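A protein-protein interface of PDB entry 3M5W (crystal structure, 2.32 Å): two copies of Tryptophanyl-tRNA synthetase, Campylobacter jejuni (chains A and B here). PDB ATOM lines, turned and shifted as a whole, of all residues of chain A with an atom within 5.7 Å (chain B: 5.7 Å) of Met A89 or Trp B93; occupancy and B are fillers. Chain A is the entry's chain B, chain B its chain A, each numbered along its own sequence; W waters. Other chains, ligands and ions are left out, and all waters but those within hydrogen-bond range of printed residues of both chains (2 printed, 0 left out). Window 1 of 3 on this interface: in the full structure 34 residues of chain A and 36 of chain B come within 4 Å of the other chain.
Hydrophobic or aromatic side chains of chain A that line the printed part of chain B: Tyr A44, Met A47, Met A89, Tyr A92, Trp A93 and Leu A130.
Hydrophobic or aromatic side chains of chain B within 4 Å of the printed part of chain A: Met B89, Tyr B92 and Trp B93.
Among the printed residues, Asp or Glu carboxylates within 4 Å of a Lys or Arg side-chain nitrogen of the other chain: Lys A86 with Glu B90 (2.6 Å).
The side-chain hydroxyl (OH) of Tyr A44 lies within hydrogen-bond range of the side-chain carboxylate (OE1) of Glu B90, 2.7 Å away.
NZ of Lys A86 is in salt-bridge range of OE1 of Glu B90 (2.6 Å).
O of Tyr A44 lies within hydrogen-bond range of NE1 of Trp B93, 3.1 Å away.
N of Gly A123 sits at hydrogen-bond distance from O of Ser B96, 3.3 Å away.
Val A88 touches none of the printed residues of chain B.
Met A89 touches just these residues of chain B: Met B89 and Trp B93.
Of the printed residues of chain B, Tyr A92 touches Tyr B92 (3.5 Å) and Trp B93 (3.7 Å).
Of the printed residues of chain B, Gly A123 touches Trp B93 (3.9 Å), Ser B96 (3.3 Å) and Gln B97 (3.3 Å).
Ser A126 touches none of the printed residues of chain B.
Of the printed residues of chain A, Glu B90 touches Tyr A44 and Lys A86.
Trp B93 touches seven residues of chain A.
The nearest residue of chain B that does not touch Met A89 is Glu B90 (4.1 Å).
Water W2 lies within hydrogen-bond range of OG of Ser B96 (2.5 Å), OH of Tyr A92 (2.9 Å) and O of Tyr B92 (3.4 Å).
Water W1 lies within hydrogen-bond range of the side-chain hydroxyl of Tyr B92 (2.7 Å) and the backbone carbonyl oxygen of Tyr A92 (3.3 Å).
Among the printed residues, merely in contact across the chains: Thr A48 with Gln B97 (3.0 Å), Gly A123 with Gln B97 (3.3 Å), Met A89 with Trp B93 (3.3 Å), Met A89 with Met B89 (3.5 Å), Trp A93 with Tyr B92 (3.5 Å), Tyr A92 with Tyr B92 (3.5 Å), Thr A48 with Trp B93 (3.6 Å), Leu A130 with Trp B93 (3.6 Å), Trp A93 with Met B89 (3.6 Å), Met A47 with Gln B97 (3.6 Å), Glu A90 with Met B89 (3.6 Å), Tyr A92 with Trp B93 (3.7 Å), Met A47 with Trp B93 (3.8 Å) and Gly A123 with Trp B93 (3.9 Å).
OG of Ser B96 sits at hydrogen-bond distance from O of Tyr B92 (3.1 Å).
The side-chain amide nitrogen (NE2) of Gln B97 is in hydrogen-bond range of the backbone carbonyl oxygen (O) of Trp B93, at 2.8 Å.
The side-chain hydroxyl (OG1) of Thr A48 sits at hydrogen-bond distance from the backbone carbonyl oxygen (O) of His A45 (2.8 Å).
Met A89 touches Trp B93, and with the chains exchanged Trp A93 touches Met B89.
Glu A90 touches Met B89, but with the chains exchanged Met A89 does not touch Glu B90 (4.1 Å).
Tyr A92 touches its own counterpart, Tyr B92.
Tyr A92 touches Trp B93, and with the chains exchanged Trp A93 touches Tyr B92.
7 positions are printed for both chains.
Of the 18 pairs that touch across the chains among the printed residues, 6 have their exchanged pair printed and touching as well.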
ATOM      1  N   TYR A  44     -13.417 -18.429  19.452  1.00  0.00           N
ATOM      2  CA  TYR A  44     -14.745 -18.456  20.096  1.00  0.00           C
ATOM      3  C   TYR A  44     -15.815 -17.947  19.146  1.00  0.00           C
ATOM      4  O   TYR A  44     -16.905 -18.497  19.104  1.00  0.00           O
ATOM      5  CB  TYR A  44     -14.834 -17.653  21.404  1.00  0.00           C
ATOM      6  CG  TYR A  44     -14.184 -18.308  22.596  1.00  0.00           C
ATOM      7  CD1 TYR A  44     -14.462 -19.619  22.957  1.00  0.00           C
ATOM      8  CD2 TYR A  44     -13.320 -17.583  23.380  1.00  0.00           C
ATOM      9  CE1 TYR A  44     -13.873 -20.166  24.115  1.00  0.00           C
ATOM     10  CE2 TYR A  44     -12.717 -18.117  24.494  1.00  0.00           C
ATOM     11  CZ  TYR A  44     -12.982 -19.383  24.862  1.00  0.00           C
ATOM     12  OH  TYR A  44     -12.326 -19.806  25.983  1.00  0.00           O
ATOM     13  N   HIS A  45     -15.513 -16.902  18.388  1.00  0.00           N
ATOM     14  CA  HIS A  45     -16.513 -16.416  17.451  1.00  0.00           C
ATOM     15  C   HIS A  45     -16.851 -17.407  16.359  1.00  0.00           C
ATOM     16  O   HIS A  45     -18.003 -17.482  15.925  1.00  0.00           O
ATOM     17  CB  HIS A  45     -16.101 -15.070  16.908  1.00  0.00           C
ATOM     18  CG  HIS A  45     -15.833 -14.077  17.995  1.00  0.00           C
ATOM     19  ND1 HIS A  45     -16.831 -13.592  18.819  1.00  0.00           N
ATOM     20  CD2 HIS A  45     -14.672 -13.528  18.435  1.00  0.00           C
ATOM     21  CE1 HIS A  45     -16.295 -12.761  19.698  1.00  0.00           C
ATOM     22  NE2 HIS A  45     -14.988 -12.709  19.492  1.00  0.00           N
ATOM     23  N   MET A  47     -17.290 -20.384  16.636  1.00  0.00           N
ATOM     24  CA  MET A  47     -18.230 -21.365  17.128  1.00  0.00           C
ATOM     25  C   MET A  47     -19.682 -21.019  16.856  1.00  0.00           C
ATOM     26  O   MET A  47     -20.574 -21.895  16.946  1.00  0.00           O
ATOM     27  CB  MET A  47     -18.043 -21.584  18.610  1.00  0.00           C
ATOM     28  CG  MET A  47     -16.691 -22.113  18.958  1.00  0.00           C
ATOM     29  SD  MET A  47     -16.584 -22.298  20.902  1.00  0.00           S
ATOM     30  CE  MET A  47     -14.651 -22.762  20.963  1.00  0.00           C
ATOM     31  N   THR A  48     -19.939 -19.747  16.565  1.00  0.00           N
ATOM     32  CA  THR A  48     -21.301 -19.355  16.251  1.00  0.00           C
ATOM     33  C   THR A  48     -21.651 -19.838  14.828  1.00  0.00           C
ATOM     34  O   THR A  48     -22.808 -20.097  14.516  1.00  0.00           O
ATOM     35  CB  THR A  48     -21.488 -17.834  16.331  1.00  0.00           C
ATOM     36  OG1 THR A  48     -20.739 -17.229  15.277  1.00  0.00           O
ATOM     37  CG2 THR A  48     -20.996 -17.288  17.658  1.00  0.00           C
ATOM     38  N   VAL A  85      -6.948 -17.768  26.376  1.00  0.00           N
ATOM     39  CA  VAL A  85      -7.084 -16.776  27.461  1.00  0.00           C
ATOM     40  C   VAL A  85      -8.522 -16.736  27.991  1.00  0.00           C
ATOM     41  O   VAL A  85      -9.393 -15.924  27.545  1.00  0.00           O
ATOM     42  CB  VAL A  85      -6.546 -15.376  27.061  1.00  0.00           C
ATOM     43  CG1 VAL A  85      -6.737 -14.369  28.193  1.00  0.00           C
ATOM     44  CG2 VAL A  85      -5.110 -15.476  26.681  1.00  0.00           C
ATOM     45  N   LYS A  86      -8.769 -17.637  28.939  1.00  0.00           N
ATOM     46  CA  LYS A  86     -10.130 -17.896  29.382  1.00  0.00           C
ATOM     47  C   LYS A  86     -10.826 -16.795  30.199  1.00  0.00           C
ATOM     48  O   LYS A  86     -12.053 -16.792  30.277  1.00  0.00           O
ATOM     49  CB  LYS A  86     -10.239 -19.296  30.016  1.00  0.00           C
ATOM     50  CG  LYS A  86     -10.235 -20.401  28.932  1.00  0.00           C
ATOM     51  CD  LYS A  86      -9.772 -21.745  29.470  1.00  0.00           C
ATOM     52  CE  LYS A  86      -9.296 -22.683  28.356  1.00  0.00           C
ATOM     53  NZ  LYS A  86     -10.309 -22.780  27.258  1.00  0.00           N
ATOM     54  N   GLU A  87     -10.056 -15.871  30.780  1.00  0.00           N
ATOM     55  CA  GLU A  87     -10.611 -14.736  31.522  1.00  0.00           C
ATOM     56  C   GLU A  87     -11.668 -14.048  30.691  1.00  0.00           C
ATOM     57  O   GLU A  87     -12.662 -13.567  31.214  1.00  0.00           O
ATOM     58  CB  GLU A  87      -9.540 -13.705  31.873  1.00  0.00           C
ATOM     59  CG  GLU A  87      -8.595 -14.135  32.990  1.00  0.00           C
ATOM     60  CD  GLU A  87      -7.690 -15.312  32.655  1.00  0.00           C
ATOM     61  OE1 GLU A  87      -7.668 -15.788  31.507  1.00  0.00           O
ATOM     62  OE2 GLU A  87      -6.949 -15.752  33.564  1.00  0.00           O
ATOM     63  N   VAL A  88     -11.456 -14.009  29.384  1.00  0.00           N
ATOM     64  CA  VAL A  88     -12.402 -13.344  28.517  1.00  0.00           C
ATOM     65  C   VAL A  88     -13.852 -13.810  28.641  1.00  0.00           C
ATOM     66  O   VAL A  88     -14.727 -12.986  28.439  1.00  0.00           O
ATOM     67  CB  VAL A  88     -12.020 -13.402  27.025  1.00  0.00           C
ATOM     68  CG1 VAL A  88     -12.499 -14.707  26.413  1.00  0.00           C
ATOM     69  CG2 VAL A  88     -12.657 -12.258  26.313  1.00  0.00           C
ATOM     70  N   MET A  89     -14.111 -15.096  28.936  1.00  0.00           N
ATOM     71  CA  MET A  89     -15.497 -15.599  29.127  1.00  0.00           C
ATOM     72  C   MET A  89     -16.209 -15.006  30.344  1.00  0.00           C
ATOM     73  O   MET A  89     -17.414 -14.749  30.353  1.00  0.00           O
ATOM     74  CB  MET A  89     -15.537 -17.106  29.334  1.00  0.00           C
ATOM     75  CG  MET A  89     -15.165 -17.884  28.122  1.00  0.00           C
ATOM     76  SD  MET A  89     -16.641 -17.922  26.868  1.00  0.00           S
ATOM     77  CE  MET A  89     -16.589 -16.181  26.021  1.00  0.00           C
ATOM     78  N   GLU A  90     -15.433 -14.866  31.390  1.00  0.00           N
ATOM     79  CA  GLU A  90     -15.903 -14.352  32.639  1.00  0.00           C
ATOM     80  C   GLU A  90     -16.235 -12.860  32.495  1.00  0.00           C
ATOM     81  O   GLU A  90     -17.305 -12.396  32.935  1.00  0.00           O
ATOM     82  CB  GLU A  90     -14.821 -14.603  33.673  1.00  0.00           C
ATOM     83  CG  GLU A  90     -15.381 -14.991  34.993  1.00  0.00           C
ATOM     84  CD  GLU A  90     -14.331 -15.071  36.051  1.00  0.00           C
ATOM     85  OE1 GLU A  90     -14.685 -15.521  37.149  1.00  0.00           O
ATOM     86  OE2 GLU A  90     -13.159 -14.723  35.774  1.00  0.00           O
ATOM     87  N   LEU A  91     -15.351 -12.124  31.819  1.00  0.00           N
ATOM     88  CA  LEU A  91     -15.577 -10.707  31.604  1.00  0.00           C
ATOM     89  C   LEU A  91     -16.836 -10.517  30.761  1.00  0.00           C
ATOM     90  O   LEU A  91     -17.582  -9.530  30.878  1.00  0.00           O
ATOM     91  CB  LEU A  91     -14.370 -10.070  30.907  1.00  0.00           C
ATOM     92  CG  LEU A  91     -14.590  -8.593  30.670  1.00  0.00           C
ATOM     93  CD1 LEU A  91     -14.734  -7.931  32.078  1.00  0.00           C
ATOM     94  CD2 LEU A  91     -13.477  -7.961  29.837  1.00  0.00           C
ATOM     95  N   TYR A  92     -17.074 -11.489  29.913  1.00  0.00           N
ATOM     96  CA  TYR A  92     -18.234 -11.501  29.023  1.00  0.00           C
ATOM     97  C   TYR A  92     -19.521 -11.580  29.851  1.00  0.00           C
ATOM     98  O   TYR A  92     -20.481 -10.855  29.589  1.00  0.00           O
ATOM     99  CB  TYR A  92     -18.099 -12.688  28.025  1.00  0.00           C
ATOM    100  CG  TYR A  92     -19.381 -13.166  27.365  1.00  0.00           C
ATOM    101  CD1 TYR A  92     -20.168 -12.313  26.610  1.00  0.00           C
ATOM    102  CD2 TYR A  92     -19.756 -14.491  27.455  1.00  0.00           C
ATOM    103  CE1 TYR A  92     -21.327 -12.766  25.999  1.00  0.00           C
ATOM    104  CE2 TYR A  92     -20.887 -14.966  26.834  1.00  0.00           C
ATOM    105  CZ  TYR A  92     -21.678 -14.108  26.105  1.00  0.00           C
ATOM    106  OH  TYR A  92     -22.831 -14.602  25.492  1.00  0.00           O
ATOM    107  N   TRP A  93     -19.543 -12.472  30.841  1.00  0.00           N
ATOM    108  CA  TRP A  93     -20.664 -12.549  31.783  1.00  0.00           C
ATOM    109  C   TRP A  93     -20.864 -11.188  32.495  1.00  0.00           C
ATOM    110  O   TRP A  93     -21.972 -10.610  32.540  1.00  0.00           O
ATOM    111  CB  TRP A  93     -20.433 -13.682  32.815  1.00  0.00           C
ATOM    112  CG  TRP A  93     -21.585 -13.776  33.807  1.00  0.00           C
ATOM    113  CD1 TRP A  93     -21.535 -13.562  35.185  1.00  0.00           C
ATOM    114  CD2 TRP A  93     -22.983 -14.014  33.490  1.00  0.00           C
ATOM    115  NE1 TRP A  93     -22.804 -13.700  35.735  1.00  0.00           N
ATOM    116  CE2 TRP A  93     -23.708 -13.971  34.725  1.00  0.00           C
ATOM    117  CE3 TRP A  93     -23.689 -14.260  32.295  1.00  0.00           C
ATOM    118  CZ2 TRP A  93     -25.112 -14.174  34.783  1.00  0.00           C
ATOM    119  CZ3 TRP A  93     -25.089 -14.461  32.350  1.00  0.00           C
ATOM    120  CH2 TRP A  93     -25.784 -14.395  33.599  1.00  0.00           C
ATOM    121  N   ILE A  94     -19.784 -10.665  33.061  1.00  0.00           N
ATOM    122  CA  ILE A  94     -19.858  -9.389  33.763  1.00  0.00           C
ATOM    123  C   ILE A  94     -20.405  -8.225  32.912  1.00  0.00           C
ATOM    124  O   ILE A  94     -21.221  -7.438  33.387  1.00  0.00           O
ATOM    125  CB  ILE A  94     -18.498  -9.064  34.320  1.00  0.00           C
ATOM    126  CG1 ILE A  94     -18.259  -9.971  35.510  1.00  0.00           C
ATOM    127  CG2 ILE A  94     -18.413  -7.634  34.756  1.00  0.00           C
ATOM    128  CD1 ILE A  94     -16.830 -10.464  35.600  1.00  0.00           C
ATOM    129  N   GLY A 123     -26.099 -17.191  20.627  1.00  0.00           N
ATOM    130  CA  GLY A 123     -24.706 -16.895  20.351  1.00  0.00           C
ATOM    131  C   GLY A 123     -24.572 -15.746  19.376  1.00  0.00           C
ATOM    132  O   GLY A 123     -23.764 -14.851  19.559  1.00  0.00           O
ATOM    133  N   SER A 126     -25.489 -12.548  21.078  1.00  0.00           N
ATOM    134  CA  SER A 126     -24.622 -12.167  22.179  1.00  0.00           C
ATOM    135  C   SER A 126     -23.197 -11.860  21.791  1.00  0.00           C
ATOM    136  O   SER A 126     -22.447 -11.320  22.586  1.00  0.00           O
ATOM    137  CB  SER A 126     -24.594 -13.274  23.221  1.00  0.00           C
ATOM    138  OG  SER A 126     -25.881 -13.531  23.706  1.00  0.00           O
ATOM    139  N   TYR A 127     -22.809 -12.226  20.583  1.00  0.00           N
ATOM    140  CA  TYR A 127     -21.407 -12.130  20.217  1.00  0.00           C
ATOM    141  C   TYR A 127     -20.816 -10.721  20.346  1.00  0.00           C
ATOM    142  O   TYR A 127     -19.658 -10.573  20.673  1.00  0.00           O
ATOM    143  CB  TYR A 127     -21.133 -12.802  18.864  1.00  0.00           C
ATOM    144  CG  TYR A 127     -21.125 -11.891  17.673  1.00  0.00           C
ATOM    145  CD1 TYR A 127     -20.039 -11.076  17.410  1.00  0.00           C
ATOM    146  CD2 TYR A 127     -22.197 -11.857  16.803  1.00  0.00           C
ATOM    147  CE1 TYR A 127     -20.025 -10.247  16.330  1.00  0.00           C
ATOM    148  CE2 TYR A 127     -22.194 -11.033  15.715  1.00  0.00           C
ATOM    149  CZ  TYR A 127     -21.105 -10.225  15.483  1.00  0.00           C
ATOM    150  OH  TYR A 127     -21.092  -9.396  14.396  1.00  0.00           O
ATOM    151  N   LEU A 130     -19.220 -10.439  23.756  1.00  0.00           N
ATOM    152  CA  LEU A 130     -17.958 -11.178  23.789  1.00  0.00           C
ATOM    153  C   LEU A 130     -16.864 -10.350  23.152  1.00  0.00           C
ATOM    154  O   LEU A 130     -15.785 -10.168  23.718  1.00  0.00           O
ATOM    155  CB  LEU A 130     -18.083 -12.508  23.036  1.00  0.00           C
ATOM    156  CG  LEU A 130     -16.848 -13.418  23.044  1.00  0.00           C
ATOM    157  CD1 LEU A 130     -16.155 -13.579  24.394  1.00  0.00           C
ATOM    158  CD2 LEU A 130     -17.290 -14.736  22.582  1.00  0.00           C
ATOM    159  N   VAL B  88     -17.848 -23.317  33.833  1.00  0.00           N
ATOM    160  CA  VAL B  88     -19.247 -23.246  33.487  1.00  0.00           C
ATOM    161  C   VAL B  88     -19.456 -22.125  32.518  1.00  0.00           C
ATOM    162  O   VAL B  88     -20.390 -22.127  31.726  1.00  0.00           O
ATOM    163  CB  VAL B  88     -20.162 -23.113  34.728  1.00  0.00           C
ATOM    164  CG1 VAL B  88     -19.974 -21.775  35.397  1.00  0.00           C
ATOM    165  CG2 VAL B  88     -21.621 -23.366  34.313  1.00  0.00           C
ATOM    166  N   MET B  89     -18.514 -21.196  32.562  1.00  0.00           N
ATOM    167  CA  MET B  89     -18.548 -19.957  31.825  1.00  0.00           C
ATOM    168  C   MET B  89     -18.346 -20.254  30.325  1.00  0.00           C
ATOM    169  O   MET B  89     -19.085 -19.817  29.471  1.00  0.00           O
ATOM    170  CB  MET B  89     -17.425 -19.102  32.413  1.00  0.00           C
ATOM    171  CG  MET B  89     -17.617 -17.623  32.345  1.00  0.00           C
ATOM    172  SD  MET B  89     -19.115 -16.995  33.407  1.00  0.00           S
ATOM    173  CE  MET B  89     -20.552 -17.370  32.178  1.00  0.00           C
ATOM    174  N   GLU B  90     -17.396 -21.113  30.039  1.00  0.00           N
ATOM    175  CA  GLU B  90     -17.083 -21.513  28.689  1.00  0.00           C
ATOM    176  C   GLU B  90     -18.167 -22.452  28.136  1.00  0.00           C
ATOM    177  O   GLU B  90     -18.439 -22.463  26.938  1.00  0.00           O
ATOM    178  CB  GLU B  90     -15.731 -22.226  28.723  1.00  0.00           C
ATOM    179  CG  GLU B  90     -15.059 -22.365  27.380  1.00  0.00           C
ATOM    180  CD  GLU B  90     -13.615 -22.866  27.476  1.00  0.00           C
ATOM    181  OE1 GLU B  90     -12.762 -22.310  26.739  1.00  0.00           O
ATOM    182  OE2 GLU B  90     -13.345 -23.793  28.295  1.00  0.00           O
ATOM    183  N   LEU B  91     -18.782 -23.259  28.995  1.00  0.00           N
ATOM    184  CA  LEU B  91     -19.859 -24.113  28.520  1.00  0.00           C
ATOM    185  C   LEU B  91     -21.100 -23.266  28.207  1.00  0.00           C
ATOM    186  O   LEU B  91     -21.815 -23.478  27.224  1.00  0.00           O
ATOM    187  CB  LEU B  91     -20.147 -25.193  29.511  1.00  0.00           C
ATOM    188  CG  LEU B  91     -21.330 -26.074  29.138  1.00  0.00           C
ATOM    189  CD1 LEU B  91     -20.996 -26.736  27.855  1.00  0.00           C
ATOM    190  CD2 LEU B  91     -21.611 -27.129  30.215  1.00  0.00           C
ATOM    191  N   TYR B  92     -21.338 -22.280  29.051  1.00  0.00           N
ATOM    192  CA  TYR B  92     -22.332 -21.269  28.757  1.00  0.00           C
ATOM    193  C   TYR B  92     -22.144 -20.772  27.288  1.00  0.00           C
ATOM    194  O   TYR B  92     -23.081 -20.798  26.477  1.00  0.00           O
ATOM    195  CB  TYR B  92     -22.172 -20.137  29.791  1.00  0.00           C
ATOM    196  CG  TYR B  92     -22.899 -18.852  29.535  1.00  0.00           C
ATOM    197  CD1 TYR B  92     -24.275 -18.807  29.273  1.00  0.00           C
ATOM    198  CD2 TYR B  92     -22.197 -17.642  29.590  1.00  0.00           C
ATOM    199  CE1 TYR B  92     -24.924 -17.557  29.053  1.00  0.00           C
ATOM    200  CE2 TYR B  92     -22.819 -16.420  29.391  1.00  0.00           C
ATOM    201  CZ  TYR B  92     -24.177 -16.375  29.119  1.00  0.00           C
ATOM    202  OH  TYR B  92     -24.719 -15.124  28.928  1.00  0.00           O
ATOM    203  N   TRP B  93     -20.936 -20.350  26.934  1.00  0.00           N
ATOM    204  CA  TRP B  93     -20.716 -19.852  25.578  1.00  0.00           C
ATOM    205  C   TRP B  93     -21.096 -20.904  24.521  1.00  0.00           C
ATOM    206  O   TRP B  93     -21.733 -20.603  23.510  1.00  0.00           O
ATOM    207  CB  TRP B  93     -19.285 -19.307  25.383  1.00  0.00           C
ATOM    208  CG  TRP B  93     -19.018 -18.909  23.941  1.00  0.00           C
ATOM    209  CD1 TRP B  93     -18.211 -19.569  23.047  1.00  0.00           C
ATOM    210  CD2 TRP B  93     -19.635 -17.830  23.200  1.00  0.00           C
ATOM    211  NE1 TRP B  93     -18.273 -18.950  21.824  1.00  0.00           N
ATOM    212  CE2 TRP B  93     -19.126 -17.880  21.889  1.00  0.00           C
ATOM    213  CE3 TRP B  93     -20.569 -16.825  23.524  1.00  0.00           C
ATOM    214  CZ2 TRP B  93     -19.524 -16.967  20.887  1.00  0.00           C
ATOM    215  CZ3 TRP B  93     -20.943 -15.906  22.548  1.00  0.00           C
ATOM    216  CH2 TRP B  93     -20.418 -15.988  21.235  1.00  0.00           C
ATOM    217  N   ILE B  94     -20.748 -22.149  24.785  1.00  0.00           N
ATOM    218  CA  ILE B  94     -21.076 -23.203  23.852  1.00  0.00           C
ATOM    219  C   ILE B  94     -22.550 -23.543  23.763  1.00  0.00           C
ATOM    220  O   ILE B  94     -23.062 -23.839  22.697  1.00  0.00           O
ATOM    221  CB  ILE B  94     -20.302 -24.482  24.150  1.00  0.00           C
ATOM    222  CG1 ILE B  94     -18.827 -24.297  23.770  1.00  0.00           C
ATOM    223  CG2 ILE B  94     -20.911 -25.621  23.309  1.00  0.00           C
ATOM    224  CD1 ILE B  94     -17.836 -24.731  24.821  1.00  0.00           C
ATOM    225  N   LEU B  95     -23.236 -23.540  24.889  1.00  0.00           N
ATOM    226  CA  LEU B  95     -24.646 -23.838  24.848  1.00  0.00           C
ATOM    227  C   LEU B  95     -25.392 -22.756  24.128  1.00  0.00           C
ATOM    228  O   LEU B  95     -26.443 -23.032  23.551  1.00  0.00           O
ATOM    229  CB  LEU B  95     -25.204 -24.037  26.254  1.00  0.00           C
ATOM    230  CG  LEU B  95     -24.563 -25.231  26.969  1.00  0.00           C
ATOM    231  CD1 LEU B  95     -25.213 -25.432  28.285  1.00  0.00           C
ATOM    232  CD2 LEU B  95     -24.620 -26.499  26.098  1.00  0.00           C
ATOM    233  N   SER B  96     -24.879 -21.523  24.161  1.00  0.00           N
ATOM    234  CA  SER B  96     -25.542 -20.402  23.461  1.00  0.00           C
ATOM    235  C   SER B  96     -25.686 -20.659  21.996  1.00  0.00           C
ATOM    236  O   SER B  96     -26.688 -20.307  21.397  1.00  0.00           O
ATOM    237  CB  SER B  96     -24.795 -19.094  23.609  1.00  0.00           C
ATOM    238  OG  SER B  96     -24.843 -18.685  24.955  1.00  0.00           O
ATOM    239  N   GLN B  97     -24.666 -21.270  21.412  1.00  0.00           N
ATOM    240  CA  GLN B  97     -24.688 -21.538  19.980  1.00  0.00           C
ATOM    241  C   GLN B  97     -25.799 -22.542  19.611  1.00  0.00           C
ATOM    242  O   GLN B  97     -26.229 -22.623  18.460  1.00  0.00           O
ATOM    243  CB  GLN B  97     -23.318 -22.036  19.523  1.00  0.00           C
ATOM    244  CG  GLN B  97     -22.149 -21.291  20.144  1.00  0.00           C
ATOM    245  CD  GLN B  97     -22.309 -19.784  20.062  1.00  0.00           C
ATOM    246  OE1 GLN B  97     -22.753 -19.249  19.056  1.00  0.00           O
ATOM    247  NE2 GLN B  97     -21.957 -19.090  21.149  1.00  0.00           N
HETATM  248  O   HOH W   1     -22.822 -13.197  29.204  1.00  0.00           O
HETATM  249  O   HOH W   2     -23.051 -17.383  26.178  1.00  0.00           O
